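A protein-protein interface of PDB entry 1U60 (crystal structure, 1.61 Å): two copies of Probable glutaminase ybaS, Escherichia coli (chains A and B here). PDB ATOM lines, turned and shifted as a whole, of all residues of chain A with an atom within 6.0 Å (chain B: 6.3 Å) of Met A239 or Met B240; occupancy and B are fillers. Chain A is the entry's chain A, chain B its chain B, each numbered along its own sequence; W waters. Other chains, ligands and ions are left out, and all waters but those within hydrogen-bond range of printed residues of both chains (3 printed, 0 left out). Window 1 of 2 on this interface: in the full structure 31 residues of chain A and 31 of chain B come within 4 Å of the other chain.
The backbone NH of Val A307 lies within hydrogen-bond range of the backbone carbonyl oxygen of Gly A255 (2.8 Å).
Water W3 bridges the backbone carbonyl oxygen of Ala B91 (2.8 Å) and the backbone carbonyl oxygen of Gly A248 (3.1 Å).
Water W2 lies within hydrogen-bond range of the backbone NH of Gly A248 (2.9 Å), the backbone NH of Ser A247 (3.1 Å) and the side-chain carboxylate of Asp B92 (3.2 Å).
Water W1 bridges the backbone carbonyl oxygen (O) of Gly B248 (3.2 Å) and the side-chain carboxylate (OE1) of Glu A237 (3.5 Å).
The backbone NH of Gly A248 lies within hydrogen-bond range of the side-chain carboxylate of Asp B92 (3.1 Å).
O of Met B239 sits close to SD of Met A240, 3.8 Å away.
O of Gly A248 lies close to O of Ala B91.
Of the 20 printed residues of chain B, 11 touch a printed residue of chain A.
Printed residues of chain B that touch a printed residue of chain A: Ala B91, Asp B92, Pro B93, Leu B235, Ala B236, Met B239, Met B240, Gly B248, Ala B251, Val B307 and Phe B308.
Hydrophobic or aromatic side chains of chain B that line the printed part of chain A: Ala B91, Pro B93, Leu B235, Ala B236, Met B239, Met B240, Ala B251, Val B307 and Phe B308.
Of the 21 printed residues of chain A, 9 touch a printed residue of chain B.
Hydrophobic or aromatic side chains of chain A that line the printed part of chain B: Pro A93, Leu A235, Ala A236, Met A239, Met A240, Val A307 and Phe A308.
Among the printed residues, no Asp or Glu carboxylate lies within 4 Å of a Lys or Arg side-chain nitrogen of the other chain.
Met A239 touches Phe B308, and with the chains exchanged Phe A308 touches Met B239.
Met A240 touches its own counterpart, Met B240.
Met A240 touches Gly B248, and with the chains exchanged Gly A248 touches Met B240.
Val A307 touches its own counterpart, Val B307.
Of the 18 pairs that touch across the chains among the printed residues, 15 have their exchanged pair printed and touching as well.
Of the printed residues of chain B, Met A239 touches Met B240 and Phe B308.
Of the printed residues of chain B, Gly A248 touches Ala B91, Asp B92 and Met B240.
Of the printed residues of chain B, Ala A251 touches Ala B236.
Of the printed residues of chain B, Phe A308 touches Leu B235 (3.5 Å), Ala B236 (3.8 Å) and Met B239 (3.8 Å).
Of the printed residues of chain A, Leu B235 touches Phe A308 (3.5 Å).
Printed residues of chain A within 4 Å of Met B240: Met A239, Met A240 and Gly A248.
Printed residues of chain A within 4 Å of Phe B308: Leu A235 (3.5 Å), Ala A236 (3.8 Å) and Met A239 (3.6 Å).
The nearest printed residue of chain B that does not touch Met A239 is Met B239 (4.2 Å).
Among the printed residues, merely in contact across the chains: Pro A93 with Pro B93, Leu A235 with Phe B308, Ala A236 with Ala B251, Ala A236 with Phe B308, Met A239 with Met B240, Met A239 with Phe B308, Met A240 with Met B240, Met A240 with Gly B248, Met A240 with Ala B251, Gly A248 with Met B240, Ala A251 with Ala B236, Val A307 with Val B307, Phe A308 with Leu B235, Phe A308 with Ala B236 and Phe A308 with Met B239.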
ATOM      1  N   PRO A  93       9.404  22.845  31.795  1.00  0.00           N
ATOM      2  CA  PRO A  93       8.692  24.013  32.332  1.00  0.00           C
ATOM      3  C   PRO A  93       7.373  23.585  33.003  1.00  0.00           C
ATOM      4  O   PRO A  93       6.772  22.548  32.654  1.00  0.00           O
ATOM      5  CB  PRO A  93       8.484  24.886  31.110  1.00  0.00           C
ATOM      6  CG  PRO A  93       8.345  23.940  30.014  1.00  0.00           C
ATOM      7  CD  PRO A  93       9.429  22.880  30.329  1.00  0.00           C
ATOM      8  N   LEU A 115      14.837  25.484  38.011  1.00  0.00           N
ATOM      9  CA  LEU A 115      14.703  26.939  38.005  1.00  0.00           C
ATOM     10  C   LEU A 115      13.409  27.505  38.561  1.00  0.00           C
ATOM     11  O   LEU A 115      13.275  28.698  38.577  1.00  0.00           O
ATOM     12  CB  LEU A 115      15.041  27.526  36.633  1.00  0.00           C
ATOM     13  CG  LEU A 115      16.345  27.088  36.002  1.00  0.00           C
ATOM     14  CD1 LEU A 115      16.602  27.831  34.683  1.00  0.00           C
ATOM     15  CD2 LEU A 115      17.565  27.292  36.958  1.00  0.00           C
ATOM     16  N   ILE A 234      22.556  23.324  31.209  1.00  0.00           N
ATOM     17  CA  ILE A 234      22.245  24.558  31.995  1.00  0.00           C
ATOM     18  C   ILE A 234      21.464  25.551  31.138  1.00  0.00           C
ATOM     19  O   ILE A 234      20.440  26.108  31.551  1.00  0.00           O
ATOM     20  CB  ILE A 234      23.475  25.229  32.502  1.00  0.00           C
ATOM     21  CG1 ILE A 234      24.223  24.316  33.445  1.00  0.00           C
ATOM     22  CG2 ILE A 234      23.121  26.546  33.172  1.00  0.00           C
ATOM     23  CD1 ILE A 234      25.632  24.782  33.680  1.00  0.00           C
ATOM     24  N   LEU A 235      21.945  25.772  29.942  1.00  0.00           N
ATOM     25  CA  LEU A 235      21.293  26.688  29.009  1.00  0.00           C
ATOM     26  C   LEU A 235      19.915  26.226  28.549  1.00  0.00           C
ATOM     27  O   LEU A 235      19.021  27.059  28.377  1.00  0.00           O
ATOM     28  CB  LEU A 235      22.210  26.923  27.794  1.00  0.00           C
ATOM     29  CG  LEU A 235      23.587  27.568  28.088  1.00  0.00           C
ATOM     30  CD1 LEU A 235      24.326  27.875  26.845  1.00  0.00           C
ATOM     31  CD2 LEU A 235      23.468  28.847  28.964  1.00  0.00           C
ATOM     32  N   ALA A 236      19.731  24.916  28.378  1.00  0.00           N
ATOM     33  CA  ALA A 236      18.432  24.375  28.027  1.00  0.00           C
ATOM     34  C   ALA A 236      17.438  24.664  29.142  1.00  0.00           C
ATOM     35  O   ALA A 236      16.311  25.133  28.880  1.00  0.00           O
ATOM     36  CB  ALA A 236      18.501  22.888  27.785  1.00  0.00           C
ATOM     37  N   GLU A 237      17.851  24.427  30.379  1.00  0.00           N
ATOM     38  CA  GLU A 237      16.971  24.692  31.514  1.00  0.00           C
ATOM     39  C   GLU A 237      16.589  26.177  31.564  1.00  0.00           C
ATOM     40  O   GLU A 237      15.400  26.502  31.809  1.00  0.00           O
ATOM     41  CB  GLU A 237      17.629  24.267  32.832  1.00  0.00           C
ATOM     42  CG  GLU A 237      17.890  22.734  33.007  1.00  0.00           C
ATOM     43  CD  GLU A 237      16.748  21.868  33.445  1.00  0.00           C
ATOM     44  OE1 GLU A 237      15.546  22.255  33.301  1.00  0.00           O
ATOM     45  OE2 GLU A 237      17.066  20.715  33.943  1.00  0.00           O
ATOM     46  N   MET A 238      17.565  27.052  31.330  1.00  0.00           N
ATOM     47  CA  MET A 238      17.319  28.485  31.279  1.00  0.00           C
ATOM     48  C   MET A 238      16.314  28.816  30.153  1.00  0.00           C
ATOM     49  O   MET A 238      15.385  29.599  30.382  1.00  0.00           O
ATOM     50  CB  MET A 238      18.613  29.257  31.069  1.00  0.00           C
ATOM     51  CG  MET A 238      19.505  29.291  32.347  1.00  0.00           C
ATOM     52  SD  MET A 238      21.194  29.833  32.024  1.00  0.00           S
ATOM     53  CE  MET A 238      20.934  31.550  31.573  1.00  0.00           C
ATOM     54  N   MET A 239      16.478  28.247  28.961  1.00  0.00           N
ATOM     55  CA  MET A 239      15.563  28.579  27.864  1.00  0.00           C
ATOM     56  C   MET A 239      14.148  28.199  28.277  1.00  0.00           C
ATOM     57  O   MET A 239      13.210  28.893  27.904  1.00  0.00           O
ATOM     58  CB  MET A 239      15.941  27.849  26.571  1.00  0.00           C
ATOM     59  CG  MET A 239      15.153  28.296  25.311  1.00  0.00           C
ATOM     60  SD  MET A 239      15.491  29.868  24.700  1.00  0.00           S
ATOM     61  CE  MET A 239      17.063  29.798  24.351  1.00  0.00           C
ATOM     62  N   MET A 240      13.979  27.100  29.014  1.00  0.00           N
ATOM     63  CA  MET A 240      12.630  26.634  29.274  1.00  0.00           C
ATOM     64  C   MET A 240      11.915  27.399  30.396  1.00  0.00           C
ATOM     65  O   MET A 240      10.710  27.537  30.382  1.00  0.00           O
ATOM     66  CB  MET A 240      12.628  25.143  29.562  1.00  0.00           C
ATOM     67  CG  MET A 240      13.249  24.287  28.475  1.00  0.00           C
ATOM     68  SD  MET A 240      12.599  24.407  26.816  1.00  0.00           S
ATOM     69  CE  MET A 240      10.825  23.983  27.136  1.00  0.00           C
ATOM     70  N   GLU A 241      12.654  27.913  31.357  1.00  0.00           N
ATOM     71  CA  GLU A 241      12.045  28.408  32.602  1.00  0.00           C
ATOM     72  C   GLU A 241      12.719  29.623  33.259  1.00  0.00           C
ATOM     73  O   GLU A 241      12.234  30.103  34.271  1.00  0.00           O
ATOM     74  CB  GLU A 241      12.061  27.232  33.598  1.00  0.00           C
ATOM     75  CG  GLU A 241      11.313  27.376  34.888  1.00  0.00           C
ATOM     76  CD  GLU A 241       9.810  27.561  34.691  1.00  0.00           C
ATOM     77  OE1 GLU A 241       9.162  26.648  34.120  1.00  0.00           O
ATOM     78  OE2 GLU A 241       9.264  28.580  35.163  1.00  0.00           O
ATOM     79  N   GLY A 242      13.816  30.126  32.694  1.00  0.00           N
ATOM     80  CA  GLY A 242      14.645  31.127  33.361  1.00  0.00           C
ATOM     81  C   GLY A 242      13.974  32.465  33.649  1.00  0.00           C
ATOM     82  O   GLY A 242      14.403  33.191  34.530  1.00  0.00           O
ATOM     83  N   SER A 247       9.153  32.942  29.960  1.00  0.00           N
ATOM     84  CA  SER A 247      10.270  32.366  29.270  1.00  0.00           C
ATOM     85  C   SER A 247      10.018  32.157  27.796  1.00  0.00           C
ATOM     86  O   SER A 247      10.886  32.383  26.959  1.00  0.00           O
ATOM     87  CB  SER A 247      10.641  31.039  29.893  1.00  0.00           C
ATOM     88  OG  SER A 247      11.059  31.201  31.250  1.00  0.00           O
ATOM     89  N   GLY A 248       8.811  31.740  27.473  1.00  0.00           N
ATOM     90  CA  GLY A 248       8.477  31.556  26.075  1.00  0.00           C
ATOM     91  C   GLY A 248       8.480  32.867  25.307  1.00  0.00           C
ATOM     92  O   GLY A 248       8.958  32.948  24.151  1.00  0.00           O
ATOM     93  N   TRP A 250      10.236  35.533  26.081  1.00  0.00           N
ATOM     94  CA  TRP A 250      11.642  35.767  25.899  1.00  0.00           C
ATOM     95  C   TRP A 250      12.291  34.968  24.780  1.00  0.00           C
ATOM     96  O   TRP A 250      13.034  35.509  23.953  1.00  0.00           O
ATOM     97  CB  TRP A 250      12.365  35.519  27.226  1.00  0.00           C
ATOM     98  CG  TRP A 250      13.811  35.889  27.217  1.00  0.00           C
ATOM     99  CD1 TRP A 250      14.867  35.052  27.020  1.00  0.00           C
ATOM    100  CD2 TRP A 250      14.374  37.202  27.421  1.00  0.00           C
ATOM    101  NE1 TRP A 250      16.056  35.743  27.087  1.00  0.00           N
ATOM    102  CE2 TRP A 250      15.778  37.073  27.307  1.00  0.00           C
ATOM    103  CE3 TRP A 250      13.837  38.469  27.635  1.00  0.00           C
ATOM    104  CZ2 TRP A 250      16.636  38.147  27.456  1.00  0.00           C
ATOM    105  CZ3 TRP A 250      14.691  39.539  27.770  1.00  0.00           C
ATOM    106  CH2 TRP A 250      16.084  39.368  27.709  1.00  0.00           C
ATOM    107  N   ALA A 251      12.012  33.675  24.714  1.00  0.00           N
ATOM    108  CA  ALA A 251      12.525  32.902  23.583  1.00  0.00           C
ATOM    109  C   ALA A 251      12.054  33.419  22.222  1.00  0.00           C
ATOM    110  O   ALA A 251      12.806  33.467  21.261  1.00  0.00           O
ATOM    111  CB  ALA A 251      12.131  31.447  23.738  1.00  0.00           C
ATOM    112  N   GLY A 255      15.405  35.088  21.896  1.00  0.00           N
ATOM    113  CA  GLY A 255      16.018  33.853  21.442  1.00  0.00           C
ATOM    114  C   GLY A 255      17.389  33.528  22.039  1.00  0.00           C
ATOM    115  O   GLY A 255      18.248  32.884  21.416  1.00  0.00           O
ATOM    116  N   LEU A 256      17.590  33.961  23.266  1.00  0.00           N
ATOM    117  CA  LEU A 256      18.777  33.582  23.986  1.00  0.00           C
ATOM    118  C   LEU A 256      18.388  33.044  25.356  1.00  0.00           C
ATOM    119  O   LEU A 256      17.482  33.573  26.010  1.00  0.00           O
ATOM    120  CB  LEU A 256      19.691  34.774  24.190  1.00  0.00           C
ATOM    121  CG  LEU A 256      20.265  35.488  22.975  1.00  0.00           C
ATOM    122  CD1 LEU A 256      20.963  36.768  23.433  1.00  0.00           C
ATOM    123  CD2 LEU A 256      21.216  34.607  22.224  1.00  0.00           C
ATOM    124  N   PRO A 257      19.091  32.016  25.818  1.00  0.00           N
ATOM    125  CA  PRO A 257      18.842  31.493  27.184  1.00  0.00           C
ATOM    126  C   PRO A 257      19.103  32.540  28.221  1.00  0.00           C
ATOM    127  O   PRO A 257      20.141  33.172  28.186  1.00  0.00           O
ATOM    128  CB  PRO A 257      19.824  30.333  27.334  1.00  0.00           C
ATOM    129  CG  PRO A 257      20.707  30.390  26.123  1.00  0.00           C
ATOM    130  CD  PRO A 257      20.161  31.285  25.117  1.00  0.00           C
ATOM    131  N   GLY A 258      18.165  32.697  29.140  1.00  0.00           N
ATOM    132  CA  GLY A 258      18.239  33.798  30.097  1.00  0.00           C
ATOM    133  C   GLY A 258      17.798  33.383  31.489  1.00  0.00           C
ATOM    134  O   GLY A 258      17.296  32.282  31.729  1.00  0.00           O
ATOM    135  N   VAL A 307      19.652  32.322  19.069  1.00  0.00           N
ATOM    136  CA  VAL A 307      20.029  30.943  18.737  1.00  0.00           C
ATOM    137  C   VAL A 307      19.087  30.281  17.701  1.00  0.00           C
ATOM    138  O   VAL A 307      19.417  29.214  17.167  1.00  0.00           O
ATOM    139  CB  VAL A 307      20.127  30.025  19.975  1.00  0.00           C
ATOM    140  CG1 VAL A 307      21.043  30.611  21.061  1.00  0.00           C
ATOM    141  CG2 VAL A 307      18.776  29.660  20.542  1.00  0.00           C
ATOM    142  N   PHE A 308      17.948  30.909  17.402  1.00  0.00           N
ATOM    143  CA  PHE A 308      17.010  30.426  16.357  1.00  0.00           C
ATOM    144  C   PHE A 308      17.248  31.037  14.976  1.00  0.00           C
ATOM    145  O   PHE A 308      16.460  30.831  14.045  1.00  0.00           O
ATOM    146  CB  PHE A 308      15.566  30.664  16.828  1.00  0.00           C
ATOM    147  CG  PHE A 308      15.283  30.048  18.208  1.00  0.00           C
ATOM    148  CD1 PHE A 308      15.468  28.676  18.403  1.00  0.00           C
ATOM    149  CD2 PHE A 308      14.869  30.813  19.264  1.00  0.00           C
ATOM    150  CE1 PHE A 308      15.230  28.099  19.636  1.00  0.00           C
ATOM    151  CE2 PHE A 308      14.674  30.233  20.547  1.00  0.00           C
ATOM    152  CZ  PHE A 308      14.863  28.862  20.716  1.00  0.00           C
ATOM    153  N   ALA B  91       3.067  32.705  23.202  1.00  0.00           N
ATOM    154  CA  ALA B  91       4.386  32.167  22.960  1.00  0.00           C
ATOM    155  C   ALA B  91       4.905  31.312  24.113  1.00  0.00           C
ATOM    156  O   ALA B  91       6.097  30.997  24.135  1.00  0.00           O
ATOM    157  CB  ALA B  91       5.353  33.326  22.647  1.00  0.00           C
ATOM    158  N   ASP B  92       4.029  30.872  25.021  1.00  0.00           N
ATOM    159  CA  ASP B  92       4.488  30.176  26.242  1.00  0.00           C
ATOM    160  C   ASP B  92       4.025  28.712  26.332  1.00  0.00           C
ATOM    161  O   ASP B  92       2.918  28.346  25.906  1.00  0.00           O
ATOM    162  CB  ASP B  92       4.023  30.919  27.480  1.00  0.00           C
ATOM    163  CG  ASP B  92       4.595  32.333  27.554  1.00  0.00           C
ATOM    164  OD1 ASP B  92       5.835  32.440  27.438  1.00  0.00           O
ATOM    165  OD2 ASP B  92       3.898  33.368  27.722  1.00  0.00           O
ATOM    166  N   PRO B  93       4.855  27.881  26.964  1.00  0.00           N
ATOM    167  CA  PRO B  93       4.465  26.508  27.236  1.00  0.00           C
ATOM    168  C   PRO B  93       3.399  26.463  28.307  1.00  0.00           C
ATOM    169  O   PRO B  93       3.283  27.383  29.149  1.00  0.00           O
ATOM    170  CB  PRO B  93       5.760  25.858  27.709  1.00  0.00           C
ATOM    171  CG  PRO B  93       6.522  27.020  28.346  1.00  0.00           C
ATOM    172  CD  PRO B  93       6.182  28.201  27.472  1.00  0.00           C
ATOM    173  N   THR B  94       2.553  25.416  28.273  1.00  0.00           N
ATOM    174  CA  THR B  94       1.435  25.313  29.225  1.00  0.00           C
ATOM    175  C   THR B  94       1.729  24.509  30.473  1.00  0.00           C
ATOM    176  O   THR B  94       1.000  24.654  31.466  1.00  0.00           O
ATOM    177  CB  THR B  94       0.217  24.644  28.559  1.00  0.00           C
ATOM    178  OG1 THR B  94       0.571  23.328  28.137  1.00  0.00           O
ATOM    179  CG2 THR B  94      -0.178  25.411  27.325  1.00  0.00           C
ATOM    180  N   SER B 113       0.051  28.684  23.553  1.00  0.00           N
ATOM    181  CA  SER B 113       0.983  28.188  22.530  1.00  0.00           C
ATOM    182  C   SER B 113       0.217  27.736  21.280  1.00  0.00           C
ATOM    183  O   SER B 113      -0.724  26.980  21.377  1.00  0.00           O
ATOM    184  CB  SER B 113       1.760  26.968  23.029  1.00  0.00           C
ATOM    185  OG  SER B 113       2.561  26.373  21.970  1.00  0.00           O
ATOM    186  N   LEU B 235      10.596  28.618  15.332  1.00  0.00           N
ATOM    187  CA  LEU B 235      11.541  27.769  16.056  1.00  0.00           C
ATOM    188  C   LEU B 235      11.440  27.945  17.572  1.00  0.00           C
ATOM    189  O   LEU B 235      11.589  26.948  18.317  1.00  0.00           O
ATOM    190  CB  LEU B 235      12.983  27.973  15.539  1.00  0.00           C
ATOM    191  CG  LEU B 235      13.165  27.702  14.042  1.00  0.00           C
ATOM    192  CD1 LEU B 235      14.583  27.880  13.624  1.00  0.00           C
ATOM    193  CD2 LEU B 235      12.632  26.323  13.648  1.00  0.00           C
ATOM    194  N   ALA B 236      11.226  29.174  18.053  1.00  0.00           N
ATOM    195  CA  ALA B 236      11.110  29.389  19.486  1.00  0.00           C
ATOM    196  C   ALA B 236       9.905  28.658  20.035  1.00  0.00           C
ATOM    197  O   ALA B 236       9.954  28.042  21.097  1.00  0.00           O
ATOM    198  CB  ALA B 236      10.973  30.887  19.800  1.00  0.00           C
ATOM    199  N   GLU B 237       8.790  28.759  19.298  1.00  0.00           N
ATOM    200  CA  GLU B 237       7.558  28.089  19.701  1.00  0.00           C
ATOM    201  C   GLU B 237       7.744  26.603  19.737  1.00  0.00           C
ATOM    202  O   GLU B 237       7.283  25.942  20.669  1.00  0.00           O
ATOM    203  CB  GLU B 237       6.382  28.425  18.703  1.00  0.00           C
ATOM    204  CG  GLU B 237       5.970  29.895  18.654  1.00  0.00           C
ATOM    205  CD  GLU B 237       4.961  30.312  19.704  1.00  0.00           C
ATOM    206  OE1 GLU B 237       4.872  29.667  20.794  1.00  0.00           O
ATOM    207  OE2 GLU B 237       4.276  31.376  19.494  1.00  0.00           O
ATOM    208  N   MET B 238       8.430  26.048  18.719  1.00  0.00           N
ATOM    209  CA  MET B 238       8.772  24.629  18.712  1.00  0.00           C
ATOM    210  C   MET B 238       9.644  24.230  19.910  1.00  0.00           C
ATOM    211  O   MET B 238       9.380  23.216  20.559  1.00  0.00           O
ATOM    212  CB  MET B 238       9.500  24.269  17.402  1.00  0.00           C
ATOM    213  CG  MET B 238       8.587  24.209  16.134  1.00  0.00           C
ATOM    214  SD  MET B 238       9.486  24.138  14.630  1.00  0.00           S
ATOM    215  CE  MET B 238      10.271  22.486  14.738  1.00  0.00           C
ATOM    216  N   MET B 239      10.657  25.017  20.213  1.00  0.00           N
ATOM    217  CA  MET B 239      11.500  24.745  21.366  1.00  0.00           C
ATOM    218  C   MET B 239      10.697  24.686  22.641  1.00  0.00           C
ATOM    219  O   MET B 239      10.963  23.828  23.471  1.00  0.00           O
ATOM    220  CB  MET B 239      12.587  25.803  21.531  1.00  0.00           C
ATOM    221  CG  MET B 239      13.597  25.511  22.653  1.00  0.00           C
ATOM    222  SD  MET B 239      14.761  24.202  22.312  1.00  0.00           S
ATOM    223  CE  MET B 239      15.157  24.553  20.875  1.00  0.00           C
ATOM    224  N   MET B 240       9.715  25.567  22.812  1.00  0.00           N
ATOM    225  CA  MET B 240       8.916  25.607  24.031  1.00  0.00           C
ATOM    226  C   MET B 240       7.927  24.467  24.211  1.00  0.00           C
ATOM    227  O   MET B 240       7.672  24.050  25.359  1.00  0.00           O
ATOM    228  CB  MET B 240       8.094  26.904  24.135  1.00  0.00           C
ATOM    229  CG  MET B 240       8.881  28.146  24.269  1.00  0.00           C
ATOM    230  SD  MET B 240       9.908  28.097  25.777  1.00  0.00           S
ATOM    231  CE  MET B 240      11.486  27.675  24.988  1.00  0.00           C
ATOM    232  N   GLU B 241       7.319  24.005  23.107  1.00  0.00           N
ATOM    233  CA  GLU B 241       6.150  23.142  23.190  1.00  0.00           C
ATOM    234  C   GLU B 241       6.048  22.038  22.131  1.00  0.00           C
ATOM    235  O   GLU B 241       5.097  21.279  22.159  1.00  0.00           O
ATOM    236  CB  GLU B 241       4.906  24.059  23.129  1.00  0.00           C
ATOM    237  CG  GLU B 241       3.534  23.453  23.437  1.00  0.00           C
ATOM    238  CD  GLU B 241       3.395  22.939  24.860  1.00  0.00           C
ATOM    239  OE1 GLU B 241       3.511  23.761  25.821  1.00  0.00           O
ATOM    240  OE2 GLU B 241       3.151  21.718  25.038  1.00  0.00           O
ATOM    241  N   GLY B 242       7.008  21.937  21.215  1.00  0.00           N
ATOM    242  CA  GLY B 242       6.927  21.024  20.092  1.00  0.00           C
ATOM    243  C   GLY B 242       6.760  19.539  20.388  1.00  0.00           C
ATOM    244  O   GLY B 242       6.221  18.777  19.596  1.00  0.00           O
ATOM    245  N   LEU B 243       7.277  19.122  21.540  1.00  0.00           N
ATOM    246  CA  LEU B 243       7.156  17.724  21.973  1.00  0.00           C
ATOM    247  C   LEU B 243       6.258  17.652  23.221  1.00  0.00           C
ATOM    248  O   LEU B 243       6.393  16.746  24.061  1.00  0.00           O
ATOM    249  CB  LEU B 243       8.540  17.082  22.180  1.00  0.00           C
ATOM    250  CG  LEU B 243       9.095  16.425  20.889  1.00  0.00           C
ATOM    251  CD1 LEU B 243       9.748  17.461  20.059  1.00  0.00           C
ATOM    252  CD2 LEU B 243      10.040  15.298  21.115  1.00  0.00           C
ATOM    253  N   TYR B 244       5.357  18.628  23.328  1.00  0.00           N
ATOM    254  CA  TYR B 244       4.373  18.687  24.385  1.00  0.00           C
ATOM    255  C   TYR B 244       5.137  18.721  25.711  1.00  0.00           C
ATOM    256  O   TYR B 244       6.014  19.537  25.859  1.00  0.00           O
ATOM    257  CB  TYR B 244       3.356  17.533  24.262  1.00  0.00           C
ATOM    258  CG  TYR B 244       2.663  17.683  22.932  1.00  0.00           C
ATOM    259  CD1 TYR B 244       1.759  18.702  22.736  1.00  0.00           C
ATOM    260  CD2 TYR B 244       3.070  16.953  21.839  1.00  0.00           C
ATOM    261  CE1 TYR B 244       1.164  18.913  21.497  1.00  0.00           C
ATOM    262  CE2 TYR B 244       2.539  17.159  20.605  1.00  0.00           C
ATOM    263  CZ  TYR B 244       1.609  18.168  20.414  1.00  0.00           C
ATOM    264  OH  TYR B 244       1.072  18.410  19.201  1.00  0.00           O
ATOM    265  N   SER B 247       9.023  18.618  25.918  1.00  0.00           N
ATOM    266  CA  SER B 247       9.825  19.579  25.153  1.00  0.00           C
ATOM    267  C   SER B 247      11.083  19.966  25.922  1.00  0.00           C
ATOM    268  O   SER B 247      12.139  20.140  25.363  1.00  0.00           O
ATOM    269  CB  SER B 247       8.964  20.826  24.850  1.00  0.00           C
ATOM    270  OG  SER B 247       7.864  20.422  24.019  1.00  0.00           O
ATOM    271  N   GLY B 248      10.936  20.158  27.209  1.00  0.00           N
ATOM    272  CA  GLY B 248      12.080  20.481  28.055  1.00  0.00           C
ATOM    273  C   GLY B 248      13.121  19.370  28.039  1.00  0.00           C
ATOM    274  O   GLY B 248      14.318  19.628  27.904  1.00  0.00           O
ATOM    275  N   ALA B 251      14.830  19.623  24.792  1.00  0.00           N
ATOM    276  CA  ALA B 251      15.781  20.737  24.784  1.00  0.00           C
ATOM    277  C   ALA B 251      17.068  20.347  25.572  1.00  0.00           C
ATOM    278  O   ALA B 251      18.192  20.620  25.161  1.00  0.00           O
ATOM    279  CB  ALA B 251      15.136  21.926  25.416  1.00  0.00           C
ATOM    280  N   VAL B 307      21.687  23.960  19.669  1.00  0.00           N
ATOM    281  CA  VAL B 307      21.726  25.423  19.700  1.00  0.00           C
ATOM    282  C   VAL B 307      22.345  26.008  20.994  1.00  0.00           C
ATOM    283  O   VAL B 307      22.669  27.226  21.045  1.00  0.00           O
ATOM    284  CB  VAL B 307      20.366  26.074  19.471  1.00  0.00           C
ATOM    285  CG1 VAL B 307      19.737  25.565  18.179  1.00  0.00           C
ATOM    286  CG2 VAL B 307      19.459  25.910  20.688  1.00  0.00           C
ATOM    287  N   PHE B 308      22.551  25.182  22.001  1.00  0.00           N
ATOM    288  CA  PHE B 308      23.142  25.670  23.265  1.00  0.00           C
ATOM    289  C   PHE B 308      24.635  25.364  23.410  1.00  0.00           C
ATOM    290  O   PHE B 308      25.211  25.438  24.506  1.00  0.00           O
ATOM    291  CB  PHE B 308      22.409  25.067  24.453  1.00  0.00           C
ATOM    292  CG  PHE B 308      20.927  25.300  24.423  1.00  0.00           C
ATOM    293  CD1 PHE B 308      20.425  26.581  24.503  1.00  0.00           C
ATOM    294  CD2 PHE B 308      20.051  24.218  24.330  1.00  0.00           C
ATOM    295  CE1 PHE B 308      19.075  26.759  24.450  1.00  0.00           C
ATOM    296  CE2 PHE B 308      18.659  24.411  24.245  1.00  0.00           C
ATOM    297  CZ  PHE B 308      18.194  25.665  24.351  1.00  0.00           C
HETATM  298  O   HOH W   1      15.583  21.809  29.834  1.00  0.00           O
HETATM  299  O   HOH W   2       7.211  30.587  29.648  1.00  0.00           O
HETATM  300  O   HOH W   3       8.001  30.909  22.024  1.00  0.00           O
